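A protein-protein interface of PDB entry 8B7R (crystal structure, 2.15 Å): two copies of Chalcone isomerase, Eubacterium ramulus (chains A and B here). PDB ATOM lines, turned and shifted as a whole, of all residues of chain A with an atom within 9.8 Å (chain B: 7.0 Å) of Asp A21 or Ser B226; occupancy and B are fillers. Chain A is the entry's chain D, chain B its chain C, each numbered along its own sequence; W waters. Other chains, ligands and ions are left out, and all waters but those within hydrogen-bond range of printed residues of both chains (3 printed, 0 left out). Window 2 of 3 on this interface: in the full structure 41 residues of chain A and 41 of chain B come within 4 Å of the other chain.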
ATOM      1  N   CYS A  17      17.061  -9.567 -19.884  1.00  0.00           N
ATOM      2  CA  CYS A  17      15.817  -9.003 -19.397  1.00  0.00           C
ATOM      3  C   CYS A  17      16.202  -7.742 -18.636  1.00  0.00           C
ATOM      4  O   CYS A  17      16.797  -7.839 -17.549  1.00  0.00           O
ATOM      5  CB  CYS A  17      15.085 -10.015 -18.520  1.00  0.00           C
ATOM      6  SG  CYS A  17      13.453  -9.441 -17.995  1.00  0.00           S
ATOM      7  N   VAL A  18      15.953  -6.579 -19.255  1.00  0.00           N
ATOM      8  CA  VAL A  18      16.624  -5.361 -18.801  1.00  0.00           C
ATOM      9  C   VAL A  18      15.963  -4.755 -17.571  1.00  0.00           C
ATOM     10  O   VAL A  18      16.567  -3.882 -16.971  1.00  0.00           O
ATOM     11  CB  VAL A  18      16.763  -4.291 -19.891  1.00  0.00           C
ATOM     12  CG1 VAL A  18      17.572  -4.827 -21.047  1.00  0.00           C
ATOM     13  CG2 VAL A  18      15.427  -3.724 -20.336  1.00  0.00           C
ATOM     14  N   SER A  19      14.768  -5.216 -17.210  1.00  0.00           N
ATOM     15  CA  SER A  19      14.097  -4.790 -15.991  1.00  0.00           C
ATOM     16  C   SER A  19      13.302  -5.963 -15.423  1.00  0.00           C
ATOM     17  O   SER A  19      12.750  -6.751 -16.179  1.00  0.00           O
ATOM     18  CB  SER A  19      13.205  -3.605 -16.279  1.00  0.00           C
ATOM     19  OG  SER A  19      12.165  -3.471 -15.311  1.00  0.00           O
ATOM     20  N   GLU A  20      13.219  -6.070 -14.094  1.00  0.00           N
ATOM     21  CA  GLU A  20      12.481  -7.153 -13.459  1.00  0.00           C
ATOM     22  C   GLU A  20      11.003  -7.024 -13.773  1.00  0.00           C
ATOM     23  O   GLU A  20      10.290  -8.021 -13.805  1.00  0.00           O
ATOM     24  CB  GLU A  20      12.752  -7.220 -11.959  1.00  0.00           C
ATOM     25  CG  GLU A  20      14.103  -7.871 -11.635  1.00  0.00           C
ATOM     26  CD  GLU A  20      14.308  -9.213 -12.290  1.00  0.00           C
ATOM     27  OE1 GLU A  20      13.395 -10.096 -12.108  1.00  0.00           O
ATOM     28  OE2 GLU A  20      15.342  -9.345 -13.071  1.00  0.00           O
ATOM     29  N   ASP A  21      10.548  -5.803 -14.051  1.00  0.00           N
ATOM     30  CA  ASP A  21       9.143  -5.609 -14.351  1.00  0.00           C
ATOM     31  C   ASP A  21       8.760  -6.205 -15.700  1.00  0.00           C
ATOM     32  O   ASP A  21       7.572  -6.363 -15.975  1.00  0.00           O
ATOM     33  CB  ASP A  21       8.783  -4.136 -14.296  1.00  0.00           C
ATOM     34  CG  ASP A  21       8.619  -3.598 -12.882  1.00  0.00           C
ATOM     35  OD1 ASP A  21       8.415  -4.411 -11.930  1.00  0.00           O
ATOM     36  OD2 ASP A  21       8.673  -2.362 -12.751  1.00  0.00           O
ATOM     37  N   TYR A  22       9.739  -6.541 -16.541  1.00  0.00           N
ATOM     38  CA  TYR A  22       9.477  -7.135 -17.839  1.00  0.00           C
ATOM     39  C   TYR A  22       9.511  -8.664 -17.787  1.00  0.00           C
ATOM     40  O   TYR A  22       9.097  -9.326 -18.742  1.00  0.00           O
ATOM     41  CB  TYR A  22      10.535  -6.665 -18.836  1.00  0.00           C
ATOM     42  CG  TYR A  22      10.551  -5.191 -19.151  1.00  0.00           C
ATOM     43  CD1 TYR A  22       9.407  -4.422 -19.125  1.00  0.00           C
ATOM     44  CD2 TYR A  22      11.717  -4.591 -19.599  1.00  0.00           C
ATOM     45  CE1 TYR A  22       9.426  -3.078 -19.491  1.00  0.00           C
ATOM     46  CE2 TYR A  22      11.761  -3.252 -19.950  1.00  0.00           C
ATOM     47  CZ  TYR A  22      10.607  -2.498 -19.918  1.00  0.00           C
ATOM     48  OH  TYR A  22      10.654  -1.179 -20.286  1.00  0.00           O
ATOM     49  N   ARG A  23       9.987  -9.229 -16.689  1.00  0.00           N
ATOM     50  CA  ARG A  23      10.294 -10.640 -16.646  1.00  0.00           C
ATOM     51  C   ARG A  23       9.041 -11.476 -16.906  1.00  0.00           C
ATOM     52  O   ARG A  23       9.075 -12.402 -17.718  1.00  0.00           O
ATOM     53  CB  ARG A  23      11.011 -10.997 -15.343  1.00  0.00           C
ATOM     54  CG  ARG A  23      11.360 -12.477 -15.254  1.00  0.00           C
ATOM     55  CD  ARG A  23      12.093 -12.821 -13.973  1.00  0.00           C
ATOM     56  NE  ARG A  23      13.393 -12.183 -13.984  1.00  0.00           N
ATOM     57  CZ  ARG A  23      14.446 -12.662 -14.604  1.00  0.00           C
ATOM     58  NH1 ARG A  23      14.405 -13.839 -15.240  1.00  0.00           N
ATOM     59  NH2 ARG A  23      15.566 -11.961 -14.548  1.00  0.00           N
ATOM     60  N   PRO A  24       7.898 -11.247 -16.251  1.00  0.00           N
ATOM     61  CA  PRO A  24       6.715 -12.068 -16.519  1.00  0.00           C
ATOM     62  C   PRO A  24       6.288 -12.040 -17.985  1.00  0.00           C
ATOM     63  O   PRO A  24       5.909 -13.063 -18.548  1.00  0.00           O
ATOM     64  CB  PRO A  24       5.634 -11.508 -15.573  1.00  0.00           C
ATOM     65  CG  PRO A  24       6.419 -10.806 -14.471  1.00  0.00           C
ATOM     66  CD  PRO A  24       7.684 -10.287 -15.158  1.00  0.00           C
ATOM     67  N   LYS A  25       6.369 -10.872 -18.610  1.00  0.00           N
ATOM     68  CA  LYS A  25       5.923 -10.713 -19.986  1.00  0.00           C
ATOM     69  C   LYS A  25       6.874 -11.405 -20.954  1.00  0.00           C
ATOM     70  O   LYS A  25       6.436 -12.081 -21.886  1.00  0.00           O
ATOM     71  CB  LYS A  25       5.829  -9.225 -20.321  1.00  0.00           C
ATOM     72  CG  LYS A  25       4.542  -8.545 -19.868  1.00  0.00           C
ATOM     73  CD  LYS A  25       4.622  -7.049 -20.013  1.00  0.00           C
ATOM     74  CE  LYS A  25       3.318  -6.341 -19.678  1.00  0.00           C
ATOM     75  NZ  LYS A  25       3.084  -6.344 -18.212  1.00  0.00           N
ATOM     76  N   LEU A  26       8.175 -11.193 -20.766  1.00  0.00           N
ATOM     77  CA  LEU A  26       9.165 -11.810 -21.637  1.00  0.00           C
ATOM     78  C   LEU A  26       9.113 -13.326 -21.509  1.00  0.00           C
ATOM     79  O   LEU A  26       9.173 -14.048 -22.507  1.00  0.00           O
ATOM     80  CB  LEU A  26      10.562 -11.283 -21.294  1.00  0.00           C
ATOM     81  CG  LEU A  26      11.706 -11.909 -22.095  1.00  0.00           C
ATOM     82  CD1 LEU A  26      11.516 -11.730 -23.599  1.00  0.00           C
ATOM     83  CD2 LEU A  26      13.038 -11.339 -21.667  1.00  0.00           C
ATOM     84  N   GLN A  27       9.031 -13.810 -20.269  1.00  0.00           N
ATOM     85  CA  GLN A  27       8.987 -15.241 -20.008  1.00  0.00           C
ATOM     86  C   GLN A  27       7.739 -15.870 -20.625  1.00  0.00           C
ATOM     87  O   GLN A  27       7.792 -16.946 -21.225  1.00  0.00           O
ATOM     88  CB  GLN A  27       9.071 -15.458 -18.509  1.00  0.00           C
ATOM     89  CG  GLN A  27       9.489 -16.860 -18.124  1.00  0.00           C
ATOM     90  CD  GLN A  27       9.944 -16.953 -16.680  1.00  0.00           C
ATOM     91  OE1 GLN A  27       9.366 -17.707 -15.886  1.00  0.00           O
ATOM     92  NE2 GLN A  27      10.968 -16.195 -16.308  1.00  0.00           N
ATOM     93  N   ARG A  68      20.136 -11.804 -18.349  1.00  0.00           N
ATOM     94  CA  ARG A  68      19.348 -12.005 -17.140  1.00  0.00           C
ATOM     95  C   ARG A  68      18.147 -12.924 -17.359  1.00  0.00           C
ATOM     96  O   ARG A  68      17.455 -13.236 -16.378  1.00  0.00           O
ATOM     97  CB  ARG A  68      18.942 -10.644 -16.561  1.00  0.00           C
ATOM     98  CG  ARG A  68      20.104  -9.955 -15.863  1.00  0.00           C
ATOM     99  CD  ARG A  68      19.904  -8.459 -15.617  1.00  0.00           C
ATOM    100  NE  ARG A  68      20.142  -7.707 -16.825  1.00  0.00           N
ATOM    101  CZ  ARG A  68      20.082  -6.385 -16.905  1.00  0.00           C
ATOM    102  NH1 ARG A  68      19.867  -5.661 -15.815  1.00  0.00           N
ATOM    103  NH2 ARG A  68      20.239  -5.794 -18.080  1.00  0.00           N
ATOM    104  N   MET A  69      17.891 -13.361 -18.607  1.00  0.00           N
ATOM    105  CA  MET A  69      16.816 -14.303 -18.852  1.00  0.00           C
ATOM    106  C   MET A  69      17.394 -15.702 -19.079  1.00  0.00           C
ATOM    107  O   MET A  69      17.250 -16.572 -18.232  1.00  0.00           O
ATOM    108  CB  MET A  69      15.957 -13.854 -20.040  1.00  0.00           C
ATOM    109  CG  MET A  69      14.754 -14.759 -20.332  1.00  0.00           C
ATOM    110  SD  MET A  69      13.691 -15.154 -18.878  1.00  0.00           S
ATOM    111  CE  MET A  69      12.745 -13.649 -18.730  1.00  0.00           C
ATOM    112  N   VAL A 100      12.144  -4.402 -26.536  1.00  0.00           N
ATOM    113  CA  VAL A 100      12.288  -3.542 -25.369  1.00  0.00           C
ATOM    114  C   VAL A 100      12.687  -4.380 -24.150  1.00  0.00           C
ATOM    115  O   VAL A 100      13.617  -4.032 -23.431  1.00  0.00           O
ATOM    116  CB  VAL A 100      10.979  -2.790 -25.115  1.00  0.00           C
ATOM    117  CG1 VAL A 100      11.056  -1.944 -23.853  1.00  0.00           C
ATOM    118  CG2 VAL A 100      10.618  -1.931 -26.309  1.00  0.00           C
ATOM    119  N   TRP A 101      11.968  -5.482 -23.935  1.00  0.00           N
ATOM    120  CA  TRP A 101      12.187  -6.349 -22.791  1.00  0.00           C
ATOM    121  C   TRP A 101      13.624  -6.873 -22.754  1.00  0.00           C
ATOM    122  O   TRP A 101      14.240  -6.952 -21.684  1.00  0.00           O
ATOM    123  CB  TRP A 101      11.182  -7.511 -22.810  1.00  0.00           C
ATOM    124  CG  TRP A 101       9.767  -7.058 -22.739  1.00  0.00           C
ATOM    125  CD1 TRP A 101       9.312  -5.855 -22.311  1.00  0.00           C
ATOM    126  CD2 TRP A 101       8.623  -7.769 -23.214  1.00  0.00           C
ATOM    127  NE1 TRP A 101       7.957  -5.761 -22.491  1.00  0.00           N
ATOM    128  CE2 TRP A 101       7.504  -6.931 -23.043  1.00  0.00           C
ATOM    129  CE3 TRP A 101       8.442  -9.023 -23.810  1.00  0.00           C
ATOM    130  CZ2 TRP A 101       6.222  -7.315 -23.424  1.00  0.00           C
ATOM    131  CZ3 TRP A 101       7.173  -9.413 -24.174  1.00  0.00           C
ATOM    132  CH2 TRP A 101       6.073  -8.568 -23.976  1.00  0.00           C
ATOM    133  N   TYR B 162       2.386 -12.008 -12.132  1.00  0.00           N
ATOM    134  CA  TYR B 162       3.368 -12.140 -11.067  1.00  0.00           C
ATOM    135  C   TYR B 162       2.612 -12.696  -9.868  1.00  0.00           C
ATOM    136  O   TYR B 162       1.918 -11.954  -9.203  1.00  0.00           O
ATOM    137  CB  TYR B 162       3.959 -10.749 -10.773  1.00  0.00           C
ATOM    138  CG  TYR B 162       5.118 -10.659  -9.801  1.00  0.00           C
ATOM    139  CD1 TYR B 162       6.431 -10.785 -10.224  1.00  0.00           C
ATOM    140  CD2 TYR B 162       4.930 -10.439  -8.457  1.00  0.00           C
ATOM    141  CE1 TYR B 162       7.512 -10.694  -9.342  1.00  0.00           C
ATOM    142  CE2 TYR B 162       5.989 -10.345  -7.556  1.00  0.00           C
ATOM    143  CZ  TYR B 162       7.294 -10.483  -8.000  1.00  0.00           C
ATOM    144  OH  TYR B 162       8.388 -10.396  -7.140  1.00  0.00           O
ATOM    145  N   GLU B 196      -3.288  -2.348  -8.778  1.00  0.00           N
ATOM    146  CA  GLU B 196      -2.107  -3.121  -9.136  1.00  0.00           C
ATOM    147  C   GLU B 196      -2.308  -4.611  -8.868  1.00  0.00           C
ATOM    148  O   GLU B 196      -1.554  -5.432  -9.388  1.00  0.00           O
ATOM    149  CB  GLU B 196      -0.897  -2.637  -8.325  1.00  0.00           C
ATOM    150  CG  GLU B 196      -0.495  -1.208  -8.617  1.00  0.00           C
ATOM    151  CD  GLU B 196      -1.313  -0.111  -7.921  1.00  0.00           C
ATOM    152  OE1 GLU B 196      -2.128  -0.434  -7.020  1.00  0.00           O
ATOM    153  OE2 GLU B 196      -1.118   1.085  -8.277  1.00  0.00           O
ATOM    154  N   PHE B 222      -0.037  -9.704  -9.202  1.00  0.00           N
ATOM    155  CA  PHE B 222       0.333  -8.395  -9.686  1.00  0.00           C
ATOM    156  C   PHE B 222       0.747  -8.524 -11.145  1.00  0.00           C
ATOM    157  O   PHE B 222       0.765  -9.609 -11.714  1.00  0.00           O
ATOM    158  CB  PHE B 222       1.455  -7.843  -8.806  1.00  0.00           C
ATOM    159  CG  PHE B 222       1.078  -7.795  -7.350  1.00  0.00           C
ATOM    160  CD1 PHE B 222       0.366  -6.723  -6.835  1.00  0.00           C
ATOM    161  CD2 PHE B 222       1.357  -8.864  -6.517  1.00  0.00           C
ATOM    162  CE1 PHE B 222      -0.025  -6.716  -5.504  1.00  0.00           C
ATOM    163  CE2 PHE B 222       0.978  -8.846  -5.185  1.00  0.00           C
ATOM    164  CZ  PHE B 222       0.292  -7.771  -4.675  1.00  0.00           C
ATOM    165  N   GLU B 223       1.058  -7.375 -11.740  1.00  0.00           N
ATOM    166  CA  GLU B 223       1.598  -7.295 -13.080  1.00  0.00           C
ATOM    167  C   GLU B 223       3.099  -7.582 -13.011  1.00  0.00           C
ATOM    168  O   GLU B 223       3.676  -8.168 -13.924  1.00  0.00           O
ATOM    169  CB  GLU B 223       1.210  -5.937 -13.661  1.00  0.00           C
ATOM    170  CG  GLU B 223       1.673  -5.721 -15.090  1.00  0.00           C
ATOM    171  CD  GLU B 223       1.275  -4.400 -15.756  1.00  0.00           C
ATOM    172  OE1 GLU B 223       0.736  -3.542 -15.048  1.00  0.00           O
ATOM    173  OE2 GLU B 223       1.500  -4.244 -17.004  1.00  0.00           O
ATOM    174  N   ASN B 224       3.730  -7.178 -11.906  1.00  0.00           N
ATOM    175  CA  ASN B 224       5.173  -7.172 -11.818  1.00  0.00           C
ATOM    176  C   ASN B 224       5.611  -6.861 -10.392  1.00  0.00           C
ATOM    177  O   ASN B 224       4.798  -6.545  -9.526  1.00  0.00           O
ATOM    178  CB  ASN B 224       5.798  -6.168 -12.798  1.00  0.00           C
ATOM    179  CG  ASN B 224       5.178  -4.789 -12.716  1.00  0.00           C
ATOM    180  OD1 ASN B 224       4.932  -4.262 -11.629  1.00  0.00           O
ATOM    181  ND2 ASN B 224       4.895  -4.212 -13.871  1.00  0.00           N
ATOM    182  N   GLN B 225       6.931  -6.997 -10.179  1.00  0.00           N
ATOM    183  CA  GLN B 225       7.588  -6.750  -8.915  1.00  0.00           C
ATOM    184  C   GLN B 225       7.224  -5.374  -8.328  1.00  0.00           C
ATOM    185  O   GLN B 225       6.993  -5.274  -7.114  1.00  0.00           O
ATOM    186  CB  GLN B 225       9.090  -6.871  -9.151  1.00  0.00           C
ATOM    187  CG  GLN B 225       9.913  -6.615  -7.896  1.00  0.00           C
ATOM    188  CD  GLN B 225      11.382  -6.781  -8.150  1.00  0.00           C
ATOM    189  OE1 GLN B 225      11.915  -7.897  -8.056  1.00  0.00           O
ATOM    190  NE2 GLN B 225      12.024  -5.653  -8.446  1.00  0.00           N
ATOM    191  N   SER B 226       7.235  -4.324  -9.165  1.00  0.00           N
ATOM    192  CA  SER B 226       6.922  -2.982  -8.695  1.00  0.00           C
ATOM    193  C   SER B 226       5.519  -2.925  -8.104  1.00  0.00           C
ATOM    194  O   SER B 226       5.291  -2.222  -7.122  1.00  0.00           O
ATOM    195  CB  SER B 226       6.992  -1.939  -9.796  1.00  0.00           C
ATOM    196  OG  SER B 226       8.278  -1.858 -10.311  1.00  0.00           O
ATOM    197  N   GLY B 227       4.572  -3.598  -8.764  1.00  0.00           N
ATOM    198  CA  GLY B 227       3.205  -3.651  -8.264  1.00  0.00           C
ATOM    199  C   GLY B 227       3.133  -4.346  -6.914  1.00  0.00           C
ATOM    200  O   GLY B 227       2.483  -3.861  -5.980  1.00  0.00           O
ATOM    201  N   TRP B 228       3.829  -5.486  -6.827  1.00  0.00           N
ATOM    202  CA  TRP B 228       3.926  -6.230  -5.587  1.00  0.00           C
ATOM    203  C   TRP B 228       4.394  -5.291  -4.464  1.00  0.00           C
ATOM    204  O   TRP B 228       3.830  -5.258  -3.372  1.00  0.00           O
ATOM    205  CB  TRP B 228       4.867  -7.428  -5.777  1.00  0.00           C
ATOM    206  CG  TRP B 228       5.091  -8.154  -4.486  1.00  0.00           C
ATOM    207  CD1 TRP B 228       4.310  -9.129  -3.938  1.00  0.00           C
ATOM    208  CD2 TRP B 228       6.115  -7.864  -3.520  1.00  0.00           C
ATOM    209  NE1 TRP B 228       4.798  -9.481  -2.706  1.00  0.00           N
ATOM    210  CE2 TRP B 228       5.903  -8.721  -2.423  1.00  0.00           C
ATOM    211  CE3 TRP B 228       7.196  -6.981  -3.494  1.00  0.00           C
ATOM    212  CZ2 TRP B 228       6.746  -8.729  -1.308  1.00  0.00           C
ATOM    213  CZ3 TRP B 228       8.025  -6.973  -2.385  1.00  0.00           C
ATOM    214  CH2 TRP B 228       7.806  -7.845  -1.311  1.00  0.00           C
ATOM    215  N   TYR B 229       5.447  -4.527  -4.738  1.00  0.00           N
ATOM    216  CA  TYR B 229       6.084  -3.716  -3.711  1.00  0.00           C
ATOM    217  C   TYR B 229       5.177  -2.557  -3.317  1.00  0.00           C
ATOM    218  O   TYR B 229       5.022  -2.259  -2.128  1.00  0.00           O
ATOM    219  CB  TYR B 229       7.450  -3.226  -4.202  1.00  0.00           C
ATOM    220  CG  TYR B 229       8.190  -2.369  -3.204  1.00  0.00           C
ATOM    221  CD1 TYR B 229       7.869  -1.027  -3.009  1.00  0.00           C
ATOM    222  CD2 TYR B 229       9.176  -2.928  -2.410  1.00  0.00           C
ATOM    223  CE1 TYR B 229       8.524  -0.257  -2.062  1.00  0.00           C
ATOM    224  CE2 TYR B 229       9.847  -2.175  -1.462  1.00  0.00           C
ATOM    225  CZ  TYR B 229       9.524  -0.836  -1.297  1.00  0.00           C
ATOM    226  OH  TYR B 229      10.206  -0.139  -0.353  1.00  0.00           O
ATOM    227  N   LYS B 230       4.586  -1.894  -4.317  1.00  0.00           N
ATOM    228  CA  LYS B 230       3.670  -0.793  -4.050  1.00  0.00           C
ATOM    229  C   LYS B 230       2.595  -1.245  -3.068  1.00  0.00           C
ATOM    230  O   LYS B 230       2.261  -0.526  -2.121  1.00  0.00           O
ATOM    231  CB  LYS B 230       3.082  -0.285  -5.368  1.00  0.00           C
ATOM    232  CG  LYS B 230       2.205   0.957  -5.294  1.00  0.00           C
ATOM    233  CD  LYS B 230       0.765   0.630  -4.966  1.00  0.00           C
ATOM    234  CE  LYS B 230      -0.225   1.792  -5.072  1.00  0.00           C
ATOM    235  NZ  LYS B 230      -1.611   1.315  -4.776  1.00  0.00           N
ATOM    236  N   VAL B 231       2.056  -2.456  -3.265  1.00  0.00           N
ATOM    237  CA  VAL B 231       0.921  -2.889  -2.480  1.00  0.00           C
ATOM    238  C   VAL B 231       1.380  -3.510  -1.175  1.00  0.00           C
ATOM    239  O   VAL B 231       0.910  -3.122  -0.113  1.00  0.00           O
ATOM    240  CB  VAL B 231       0.034  -3.844  -3.274  1.00  0.00           C
ATOM    241  CG1 VAL B 231      -1.114  -4.365  -2.431  1.00  0.00           C
ATOM    242  CG2 VAL B 231      -0.488  -3.159  -4.534  1.00  0.00           C
ATOM    243  N   MET B 232       2.299  -4.470  -1.262  1.00  0.00           N
ATOM    244  CA  MET B 232       2.615  -5.328  -0.127  1.00  0.00           C
ATOM    245  C   MET B 232       3.570  -4.636   0.851  1.00  0.00           C
ATOM    246  O   MET B 232       3.656  -5.037   2.025  1.00  0.00           O
ATOM    247  CB  MET B 232       3.223  -6.644  -0.600  1.00  0.00           C
ATOM    248  CG  MET B 232       2.300  -7.425  -1.523  1.00  0.00           C
ATOM    249  SD  MET B 232       0.772  -7.859  -0.711  1.00  0.00           S
ATOM    250  CE  MET B 232       1.319  -9.172   0.370  1.00  0.00           C
ATOM    251  N   ASP B 234       4.300  -0.583   0.460  1.00  0.00           N
ATOM    252  CA  ASP B 234       3.836   0.782   0.667  1.00  0.00           C
ATOM    253  C   ASP B 234       2.377   0.842   1.145  1.00  0.00           C
ATOM    254  O   ASP B 234       2.091   1.495   2.137  1.00  0.00           O
ATOM    255  CB  ASP B 234       4.084   1.648  -0.570  1.00  0.00           C
ATOM    256  CG  ASP B 234       5.542   2.020  -0.785  1.00  0.00           C
ATOM    257  OD1 ASP B 234       6.343   1.980   0.214  1.00  0.00           O
ATOM    258  OD2 ASP B 234       5.884   2.332  -1.952  1.00  0.00           O
HETATM  259  O   HOH W   1       3.008  -8.711 -16.485  1.00  0.00           O
HETATM  260  O   HOH W   2       8.321  -8.527 -12.215  1.00  0.00           O
HETATM  261  O   HOH W   3       5.163  -5.066 -16.610  1.00  0.00           O
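The side-chain amino group (NZ) of Lys A25 lies within salt-bridge range of the side-chain carboxylate (OE2) of Glu B223, at 2.9 Å. The side-chain amide oxygen (OD1) of Asn B224 sits close to the side-chain carboxylate (OD1) of Asp A21. The backbone NH of Gln B225 sits at hydrogen-bond distance from the side-chain carboxylate of Asp A21 (3.5 Å). The side-chain hydroxyl (OG) of Ser B226 lies within hydrogen-bond range of the side-chain carboxylate (OD2) of Asp A21 (2.5 Å).
OD1 of Asn B224 sits close to N of Ser B226, at 3.4 Å. The backbone NH of Gly B227 is in hydrogen-bond range of the side-chain amide oxygen of Asn B224 (3.0 Å). N of Asp A21 lies close to OG of Ser A19. The guanidinium group of Arg A23 lies within salt-bridge range of the side-chain carboxylate of Glu A20 (2.8 Å).
Among the printed residues, merely in contact across the chains: Glu A20 with Gln B225 (3.9 Å) and Pro A24 with Glu B223 (3.8 Å).
Val A18 touches none of the printed residues of chain B. Printed residues of chain B within 4 Å of Glu A20: Gln B225 (3.9 Å). Printed residues of chain B within 4 Å of Pro A24: Glu B223. Of the printed residues of chain B, Lys A25 touches Glu B223 (2.9 Å). Val A100 touches none of the printed residues of chain B. Printed residues of chain A within 4 Å of Glu B223: Pro A24 (3.8 Å) and Lys A25 (2.9 Å). Of chain A, only Asp A21 (3.3 Å) comes within 4 Å of Asn B224. Of the printed residues of chain A, Gln B225 touches Glu A20 and Asp A21. Ser B226 touches one residue of chain A. No residue of chain A comes within 4 Å of Gly B227. The nearest residue of chain B that does not touch Asp A21 is Glu B223 (4.8 Å). The nearest printed residue of chain A that does not touch Ser B226 is Ser A19 (6.5 Å).
Of the 14 printed residues of chain B, 4 touch a printed residue of chain A. Printed residues of chain B that touch a printed residue of chain A: Glu B223, Asn B224, Gln B225 and Ser B226. Among the printed residues, 6 pairs touch across the chains.
No position is printed for both chains.
Water W2 bridges O of Glu A20 and N of Gln B225. Water W1 bridges O of Glu B223 (2.7 Å) and NZ of Lys A25 (2.9 Å). Water W3 lies within hydrogen-bond range of the backbone carbonyl oxygen (O) of Asp A21 (2.8 Å), the side-chain amide nitrogen (ND2) of Asn B224 (2.9 Å) and the side-chain amino group (NZ) of Lys A25 (2.9 Å).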
